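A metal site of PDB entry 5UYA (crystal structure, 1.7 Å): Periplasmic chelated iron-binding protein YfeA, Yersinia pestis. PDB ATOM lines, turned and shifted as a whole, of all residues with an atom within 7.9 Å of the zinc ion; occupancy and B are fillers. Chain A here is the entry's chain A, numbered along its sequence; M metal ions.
OE2 of Glu 207 lies close to N of Asn 228, 2.9 Å away.
The backbone NH of His 76 lies within hydrogen-bond range of the side-chain carboxylate of Glu 74 (2.8 Å).
ND2 of Asn 228 is in hydrogen-bond range of OE2 of Glu 74 (3.1 Å).
The backbone NH (N) of Glu 207 sits at hydrogen-bond distance from the side-chain carboxylate (OE1) of Glu 256, at 2.8 Å.
The side-chain amide oxygen (OD1) of Asn 228 lies within hydrogen-bond range of the indole nitrogen (NE1) of Trp 225 (2.9 Å).
The side-chain amide oxygen (OD1) of Asn 139 is in hydrogen-bond range of a ring nitrogen (ND1) of His 141 (2.8 Å).
ND2 of Asn 228 lies close to OD2 of Asp 282 (3.4 Å).
Asn 228 touches the zinc ion.
Five residues have an atom within 4 Å of the zinc ion: His 76, His 141, Glu 207, Asn 228 and Asp 282.
The zinc ion is bound by a ring nitrogen (NE2) of His 76 (2.1 Å), the side-chain carboxylate (OE1) of Glu 207 (2.1 Å), a ring nitrogen (NE2) of His 141 (2.2 Å), the side-chain carboxylate (OD2) of Asp 282 (2.2 Å), the side-chain carboxylate (OD1) of Asp 282 (2.5 Å) and the side-chain carboxylate (OE2) of Glu 207 (2.6 Å).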
ATOM      1  N   GLU A  74      14.144   0.866 -25.050  1.00  0.00           N
ATOM      2  CA  GLU A  74      14.631  -0.504 -24.912  1.00  0.00           C
ATOM      3  C   GLU A  74      15.639  -0.586 -23.767  1.00  0.00           C
ATOM      4  O   GLU A  74      16.618   0.159 -23.745  1.00  0.00           O
ATOM      5  CB  GLU A  74      15.259  -0.948 -26.231  1.00  0.00           C
ATOM      6  CG  GLU A  74      15.340  -2.457 -26.424  1.00  0.00           C
ATOM      7  CD  GLU A  74      16.302  -3.113 -25.458  1.00  0.00           C
ATOM      8  OE1 GLU A  74      17.503  -2.771 -25.504  1.00  0.00           O
ATOM      9  OE2 GLU A  74      15.851  -3.965 -24.668  1.00  0.00           O
ATOM     10  N   ILE A  75      15.402  -1.502 -22.824  1.00  0.00           N
ATOM     11  CA  ILE A  75      16.133  -1.483 -21.552  1.00  0.00           C
ATOM     12  C   ILE A  75      17.336  -2.419 -21.496  1.00  0.00           C
ATOM     13  O   ILE A  75      18.219  -2.197 -20.658  1.00  0.00           O
ATOM     14  CB  ILE A  75      15.184  -1.779 -20.371  1.00  0.00           C
ATOM     15  CG1 ILE A  75      14.728  -3.244 -20.357  1.00  0.00           C
ATOM     16  CG2 ILE A  75      13.982  -0.847 -20.389  1.00  0.00           C
ATOM     17  CD1 ILE A  75      13.820  -3.575 -19.170  1.00  0.00           C
ATOM     18  N   HIS A  76      17.393  -3.451 -22.327  1.00  0.00           N
ATOM     19  CA  HIS A  76      18.468  -4.427 -22.174  1.00  0.00           C
ATOM     20  C   HIS A  76      19.806  -3.846 -22.604  1.00  0.00           C
ATOM     21  O   HIS A  76      20.815  -4.011 -21.920  1.00  0.00           O
ATOM     22  CB  HIS A  76      18.161  -5.680 -22.989  1.00  0.00           C
ATOM     23  CG  HIS A  76      16.960  -6.436 -22.538  1.00  0.00           C
ATOM     24  ND1 HIS A  76      17.056  -7.641 -21.853  1.00  0.00           N
ATOM     25  CD2 HIS A  76      15.625  -6.202 -22.685  1.00  0.00           C
ATOM     26  CE1 HIS A  76      15.846  -8.092 -21.590  1.00  0.00           C
ATOM     27  NE2 HIS A  76      14.956  -7.253 -22.094  1.00  0.00           N
ATOM     28  N   LEU A 101      19.528  -8.432 -16.709  1.00  0.00           N
ATOM     29  CA  LEU A 101      18.632  -7.550 -17.452  1.00  0.00           C
ATOM     30  C   LEU A 101      19.414  -6.374 -18.038  1.00  0.00           C
ATOM     31  O   LEU A 101      19.504  -6.221 -19.256  1.00  0.00           O
ATOM     32  CB  LEU A 101      17.502  -7.025 -16.550  1.00  0.00           C
ATOM     33  CG  LEU A 101      16.578  -6.045 -17.298  1.00  0.00           C
ATOM     34  CD1 LEU A 101      15.785  -6.732 -18.433  1.00  0.00           C
ATOM     35  CD2 LEU A 101      15.644  -5.335 -16.338  1.00  0.00           C
ATOM     36  N   ASN A 139      16.736 -15.872 -17.129  1.00  0.00           N
ATOM     37  CA  ASN A 139      15.805 -14.975 -17.816  1.00  0.00           C
ATOM     38  C   ASN A 139      15.478 -13.822 -16.867  1.00  0.00           C
ATOM     39  O   ASN A 139      15.020 -14.072 -15.746  1.00  0.00           O
ATOM     40  CB  ASN A 139      14.548 -15.762 -18.230  1.00  0.00           C
ATOM     41  CG  ASN A 139      13.555 -14.933 -19.044  1.00  0.00           C
ATOM     42  OD1 ASN A 139      13.343 -13.746 -18.797  1.00  0.00           O
ATOM     43  ND2 ASN A 139      12.900 -15.596 -19.995  1.00  0.00           N
ATOM     44  N   PRO A 140      15.713 -12.564 -17.261  1.00  0.00           N
ATOM     45  CA  PRO A 140      15.556 -11.460 -16.293  1.00  0.00           C
ATOM     46  C   PRO A 140      14.114 -11.062 -15.974  1.00  0.00           C
ATOM     47  O   PRO A 140      13.906 -10.357 -14.977  1.00  0.00           O
ATOM     48  CB  PRO A 140      16.273 -10.299 -16.991  1.00  0.00           C
ATOM     49  CG  PRO A 140      16.091 -10.572 -18.453  1.00  0.00           C
ATOM     50  CD  PRO A 140      16.231 -12.101 -18.558  1.00  0.00           C
ATOM     51  N   HIS A 141      13.135 -11.473 -16.777  1.00  0.00           N
ATOM     52  CA  HIS A 141      11.806 -10.869 -16.718  1.00  0.00           C
ATOM     53  C   HIS A 141      10.946 -11.427 -15.585  1.00  0.00           C
ATOM     54  O   HIS A 141       9.781 -11.753 -15.789  1.00  0.00           O
ATOM     55  CB  HIS A 141      11.088 -11.050 -18.060  1.00  0.00           C
ATOM     56  CG  HIS A 141      11.837 -10.513 -19.249  1.00  0.00           C
ATOM     57  ND1 HIS A 141      12.662 -11.306 -20.016  1.00  0.00           N
ATOM     58  CD2 HIS A 141      11.855  -9.288 -19.819  1.00  0.00           C
ATOM     59  CE1 HIS A 141      13.173 -10.580 -21.001  1.00  0.00           C
ATOM     60  NE2 HIS A 141      12.691  -9.345 -20.903  1.00  0.00           N
ATOM     61  N   TRP A 143       9.466 -10.177 -13.076  1.00  0.00           N
ATOM     62  CA  TRP A 143       8.330  -9.382 -12.590  1.00  0.00           C
ATOM     63  C   TRP A 143       7.018  -9.740 -13.278  1.00  0.00           C
ATOM     64  O   TRP A 143       5.974  -9.237 -12.835  1.00  0.00           O
ATOM     65  CB  TRP A 143       8.626  -7.882 -12.786  1.00  0.00           C
ATOM     66  CG  TRP A 143       8.830  -7.476 -14.226  1.00  0.00           C
ATOM     67  CD1 TRP A 143       7.862  -7.084 -15.114  1.00  0.00           C
ATOM     68  CD2 TRP A 143      10.077  -7.405 -14.917  1.00  0.00           C
ATOM     69  NE1 TRP A 143       8.442  -6.796 -16.340  1.00  0.00           N
ATOM     70  CE2 TRP A 143       9.807  -6.983 -16.237  1.00  0.00           C
ATOM     71  CE3 TRP A 143      11.408  -7.655 -14.543  1.00  0.00           C
ATOM     72  CZ2 TRP A 143      10.802  -6.798 -17.190  1.00  0.00           C
ATOM     73  CZ3 TRP A 143      12.398  -7.490 -15.488  1.00  0.00           C
ATOM     74  CH2 TRP A 143      12.097  -7.070 -16.799  1.00  0.00           C
ATOM     75  N   GLU A 207       9.973 -11.072 -28.256  1.00  0.00           N
ATOM     76  CA  GLU A 207      10.946 -11.487 -27.255  1.00  0.00           C
ATOM     77  C   GLU A 207      10.334 -12.565 -26.365  1.00  0.00           C
ATOM     78  O   GLU A 207       9.152 -12.524 -26.040  1.00  0.00           O
ATOM     79  CB  GLU A 207      11.381 -10.282 -26.393  1.00  0.00           C
ATOM     80  CG  GLU A 207      12.456 -10.658 -25.348  1.00  0.00           C
ATOM     81  CD  GLU A 207      12.855  -9.515 -24.397  1.00  0.00           C
ATOM     82  OE1 GLU A 207      12.027  -8.630 -24.080  1.00  0.00           O
ATOM     83  OE2 GLU A 207      14.009  -9.528 -23.946  1.00  0.00           O
ATOM     84  N   GLY A 208      11.172 -13.527 -25.957  1.00  0.00           N
ATOM     85  CA  GLY A 208      10.751 -14.553 -24.999  1.00  0.00           C
ATOM     86  C   GLY A 208      10.745 -14.013 -23.582  1.00  0.00           C
ATOM     87  O   GLY A 208      11.360 -14.596 -22.681  1.00  0.00           O
ATOM     88  N   ALA A 209      10.030 -12.910 -23.381  1.00  0.00           N
ATOM     89  CA  ALA A 209      10.025 -12.153 -22.139  1.00  0.00           C
ATOM     90  C   ALA A 209       8.989 -12.630 -21.140  1.00  0.00           C
ATOM     91  O   ALA A 209       8.893 -12.061 -20.050  1.00  0.00           O
ATOM     92  CB  ALA A 209       9.765 -10.669 -22.422  1.00  0.00           C
ATOM     93  N   PHE A 210       8.196 -13.652 -21.494  1.00  0.00           N
ATOM     94  CA  PHE A 210       7.005 -13.992 -20.741  1.00  0.00           C
ATOM     95  C   PHE A 210       7.120 -15.346 -20.046  1.00  0.00           C
ATOM     96  O   PHE A 210       6.120 -15.894 -19.583  1.00  0.00           O
ATOM     97  CB  PHE A 210       5.785 -13.929 -21.664  1.00  0.00           C
ATOM     98  CG  PHE A 210       5.580 -12.556 -22.241  1.00  0.00           C
ATOM     99  CD1 PHE A 210       4.892 -11.592 -21.521  1.00  0.00           C
ATOM    100  CD2 PHE A 210       6.133 -12.221 -23.471  1.00  0.00           C
ATOM    101  CE1 PHE A 210       4.737 -10.304 -22.025  1.00  0.00           C
ATOM    102  CE2 PHE A 210       5.968 -10.946 -23.990  1.00  0.00           C
ATOM    103  CZ  PHE A 210       5.279  -9.972 -23.272  1.00  0.00           C
ATOM    104  N   TRP A 225      12.723 -14.340 -30.635  1.00  0.00           N
ATOM    105  CA  TRP A 225      14.098 -14.331 -30.142  1.00  0.00           C
ATOM    106  C   TRP A 225      14.067 -14.471 -28.623  1.00  0.00           C
ATOM    107  O   TRP A 225      13.145 -13.953 -27.984  1.00  0.00           O
ATOM    108  CB  TRP A 225      14.871 -13.076 -30.544  1.00  0.00           C
ATOM    109  CG  TRP A 225      14.225 -11.778 -30.188  1.00  0.00           C
ATOM    110  CD1 TRP A 225      14.364 -11.077 -29.019  1.00  0.00           C
ATOM    111  CD2 TRP A 225      13.336 -10.999 -31.011  1.00  0.00           C
ATOM    112  NE1 TRP A 225      13.622  -9.916 -29.071  1.00  0.00           N
ATOM    113  CE2 TRP A 225      12.982  -9.843 -30.279  1.00  0.00           C
ATOM    114  CE3 TRP A 225      12.809 -11.162 -32.302  1.00  0.00           C
ATOM    115  CZ2 TRP A 225      12.123  -8.859 -30.789  1.00  0.00           C
ATOM    116  CZ3 TRP A 225      11.965 -10.185 -32.808  1.00  0.00           C
ATOM    117  CH2 TRP A 225      11.625  -9.045 -32.057  1.00  0.00           C
ATOM    118  N   PRO A 226      15.030 -15.175 -28.029  1.00  0.00           N
ATOM    119  CA  PRO A 226      14.910 -15.500 -26.590  1.00  0.00           C
ATOM    120  C   PRO A 226      15.073 -14.278 -25.683  1.00  0.00           C
ATOM    121  O   PRO A 226      14.433 -14.224 -24.633  1.00  0.00           O
ATOM    122  CB  PRO A 226      16.007 -16.541 -26.352  1.00  0.00           C
ATOM    123  CG  PRO A 226      16.985 -16.342 -27.456  1.00  0.00           C
ATOM    124  CD  PRO A 226      16.194 -15.836 -28.651  1.00  0.00           C
ATOM    125  N   ILE A 227      15.910 -13.315 -26.046  1.00  0.00           N
ATOM    126  CA  ILE A 227      16.095 -12.116 -25.234  1.00  0.00           C
ATOM    127  C   ILE A 227      16.592 -11.014 -26.150  1.00  0.00           C
ATOM    128  O   ILE A 227      17.332 -11.276 -27.108  1.00  0.00           O
ATOM    129  CB  ILE A 227      17.055 -12.389 -24.037  1.00  0.00           C
ATOM    130  CG1 ILE A 227      17.164 -11.169 -23.104  1.00  0.00           C
ATOM    131  CG2 ILE A 227      18.450 -12.799 -24.530  1.00  0.00           C
ATOM    132  CD1 ILE A 227      17.800 -11.513 -21.744  1.00  0.00           C
ATOM    133  N   ASN A 228      16.158  -9.786 -25.873  1.00  0.00           N
ATOM    134  CA  ASN A 228      16.575  -8.657 -26.693  1.00  0.00           C
ATOM    135  C   ASN A 228      18.097  -8.600 -26.766  1.00  0.00           C
ATOM    136  O   ASN A 228      18.788  -8.687 -25.750  1.00  0.00           O
ATOM    137  CB  ASN A 228      16.031  -7.343 -26.115  1.00  0.00           C
ATOM    138  CG  ASN A 228      14.513  -7.214 -26.284  1.00  0.00           C
ATOM    139  OD1 ASN A 228      13.858  -8.057 -26.898  1.00  0.00           O
ATOM    140  ND2 ASN A 228      13.942  -6.141 -25.730  1.00  0.00           N
ATOM    141  N   GLU A 256       5.754  -6.650 -28.475  1.00  0.00           N
ATOM    142  CA  GLU A 256       5.900  -5.991 -27.189  1.00  0.00           C
ATOM    143  C   GLU A 256       6.261  -4.527 -27.396  1.00  0.00           C
ATOM    144  O   GLU A 256       6.746  -4.132 -28.459  1.00  0.00           O
ATOM    145  CB  GLU A 256       6.959  -6.660 -26.311  1.00  0.00           C
ATOM    146  CG  GLU A 256       6.680  -8.148 -26.055  1.00  0.00           C
ATOM    147  CD  GLU A 256       7.260  -9.028 -27.128  1.00  0.00           C
ATOM    148  OE1 GLU A 256       8.478  -8.873 -27.400  1.00  0.00           O
ATOM    149  OE2 GLU A 256       6.515  -9.853 -27.697  1.00  0.00           O
ATOM    150  N   THR A 258       8.452  -2.201 -26.487  1.00  0.00           N
ATOM    151  CA  THR A 258       9.721  -1.517 -26.734  1.00  0.00           C
ATOM    152  C   THR A 258      10.450  -1.999 -27.977  1.00  0.00           C
ATOM    153  O   THR A 258      11.546  -1.501 -28.247  1.00  0.00           O
ATOM    154  CB  THR A 258      10.695  -1.635 -25.533  1.00  0.00           C
ATOM    155  OG1 THR A 258      11.152  -2.989 -25.402  1.00  0.00           O
ATOM    156  CG2 THR A 258      10.048  -1.176 -24.241  1.00  0.00           C
ATOM    157  N   ILE A 259       9.902  -2.955 -28.735  1.00  0.00           N
ATOM    158  CA  ILE A 259      10.563  -3.515 -29.902  1.00  0.00           C
ATOM    159  C   ILE A 259       9.632  -3.383 -31.110  1.00  0.00           C
ATOM    160  O   ILE A 259       8.484  -2.954 -30.999  1.00  0.00           O
ATOM    161  CB  ILE A 259      11.016  -4.965 -29.671  1.00  0.00           C
ATOM    162  CG1 ILE A 259       9.870  -5.808 -29.102  1.00  0.00           C
ATOM    163  CG2 ILE A 259      12.202  -4.995 -28.709  1.00  0.00           C
ATOM    164  CD1 ILE A 259       8.952  -6.407 -30.173  1.00  0.00           C
ATOM    165  N   VAL A 281       5.850  -5.468 -21.159  1.00  0.00           N
ATOM    166  CA  VAL A 281       6.704  -6.248 -20.262  1.00  0.00           C
ATOM    167  C   VAL A 281       7.916  -5.422 -19.826  1.00  0.00           C
ATOM    168  O   VAL A 281       8.207  -5.322 -18.632  1.00  0.00           O
ATOM    169  CB  VAL A 281       7.139  -7.576 -20.911  1.00  0.00           C
ATOM    170  CG1 VAL A 281       7.636  -7.392 -22.350  1.00  0.00           C
ATOM    171  CG2 VAL A 281       8.211  -8.274 -20.034  1.00  0.00           C
ATOM    172  N   ASP A 282       8.613  -4.804 -20.789  1.00  0.00           N
ATOM    173  CA  ASP A 282       9.870  -4.153 -20.466  1.00  0.00           C
ATOM    174  C   ASP A 282       9.695  -2.694 -20.074  1.00  0.00           C
ATOM    175  O   ASP A 282      10.650  -2.090 -19.572  1.00  0.00           O
ATOM    176  CB  ASP A 282      10.823  -4.225 -21.662  1.00  0.00           C
ATOM    177  CG  ASP A 282      11.555  -5.576 -21.768  1.00  0.00           C
ATOM    178  OD1 ASP A 282      11.337  -6.464 -20.919  1.00  0.00           O
ATOM    179  OD2 ASP A 282      12.344  -5.721 -22.725  1.00  0.00           O
ATOM    180  N   SER A 283       8.498  -2.118 -20.283  1.00  0.00           N
ATOM    181  CA  SER A 283       8.283  -0.714 -19.950  1.00  0.00           C
ATOM    182  C   SER A 283       6.808  -0.453 -19.699  1.00  0.00           C
ATOM    183  O   SER A 283       5.935  -1.096 -20.311  1.00  0.00           O
ATOM    184  CB  SER A 283       8.795   0.193 -21.077  1.00  0.00           C
ATOM    185  OG  SER A 283       8.644   1.578 -20.721  1.00  0.00           O
HETATM  186 ZN    ZN M   1      12.940  -7.779 -22.376  1.00  0.00          ZN
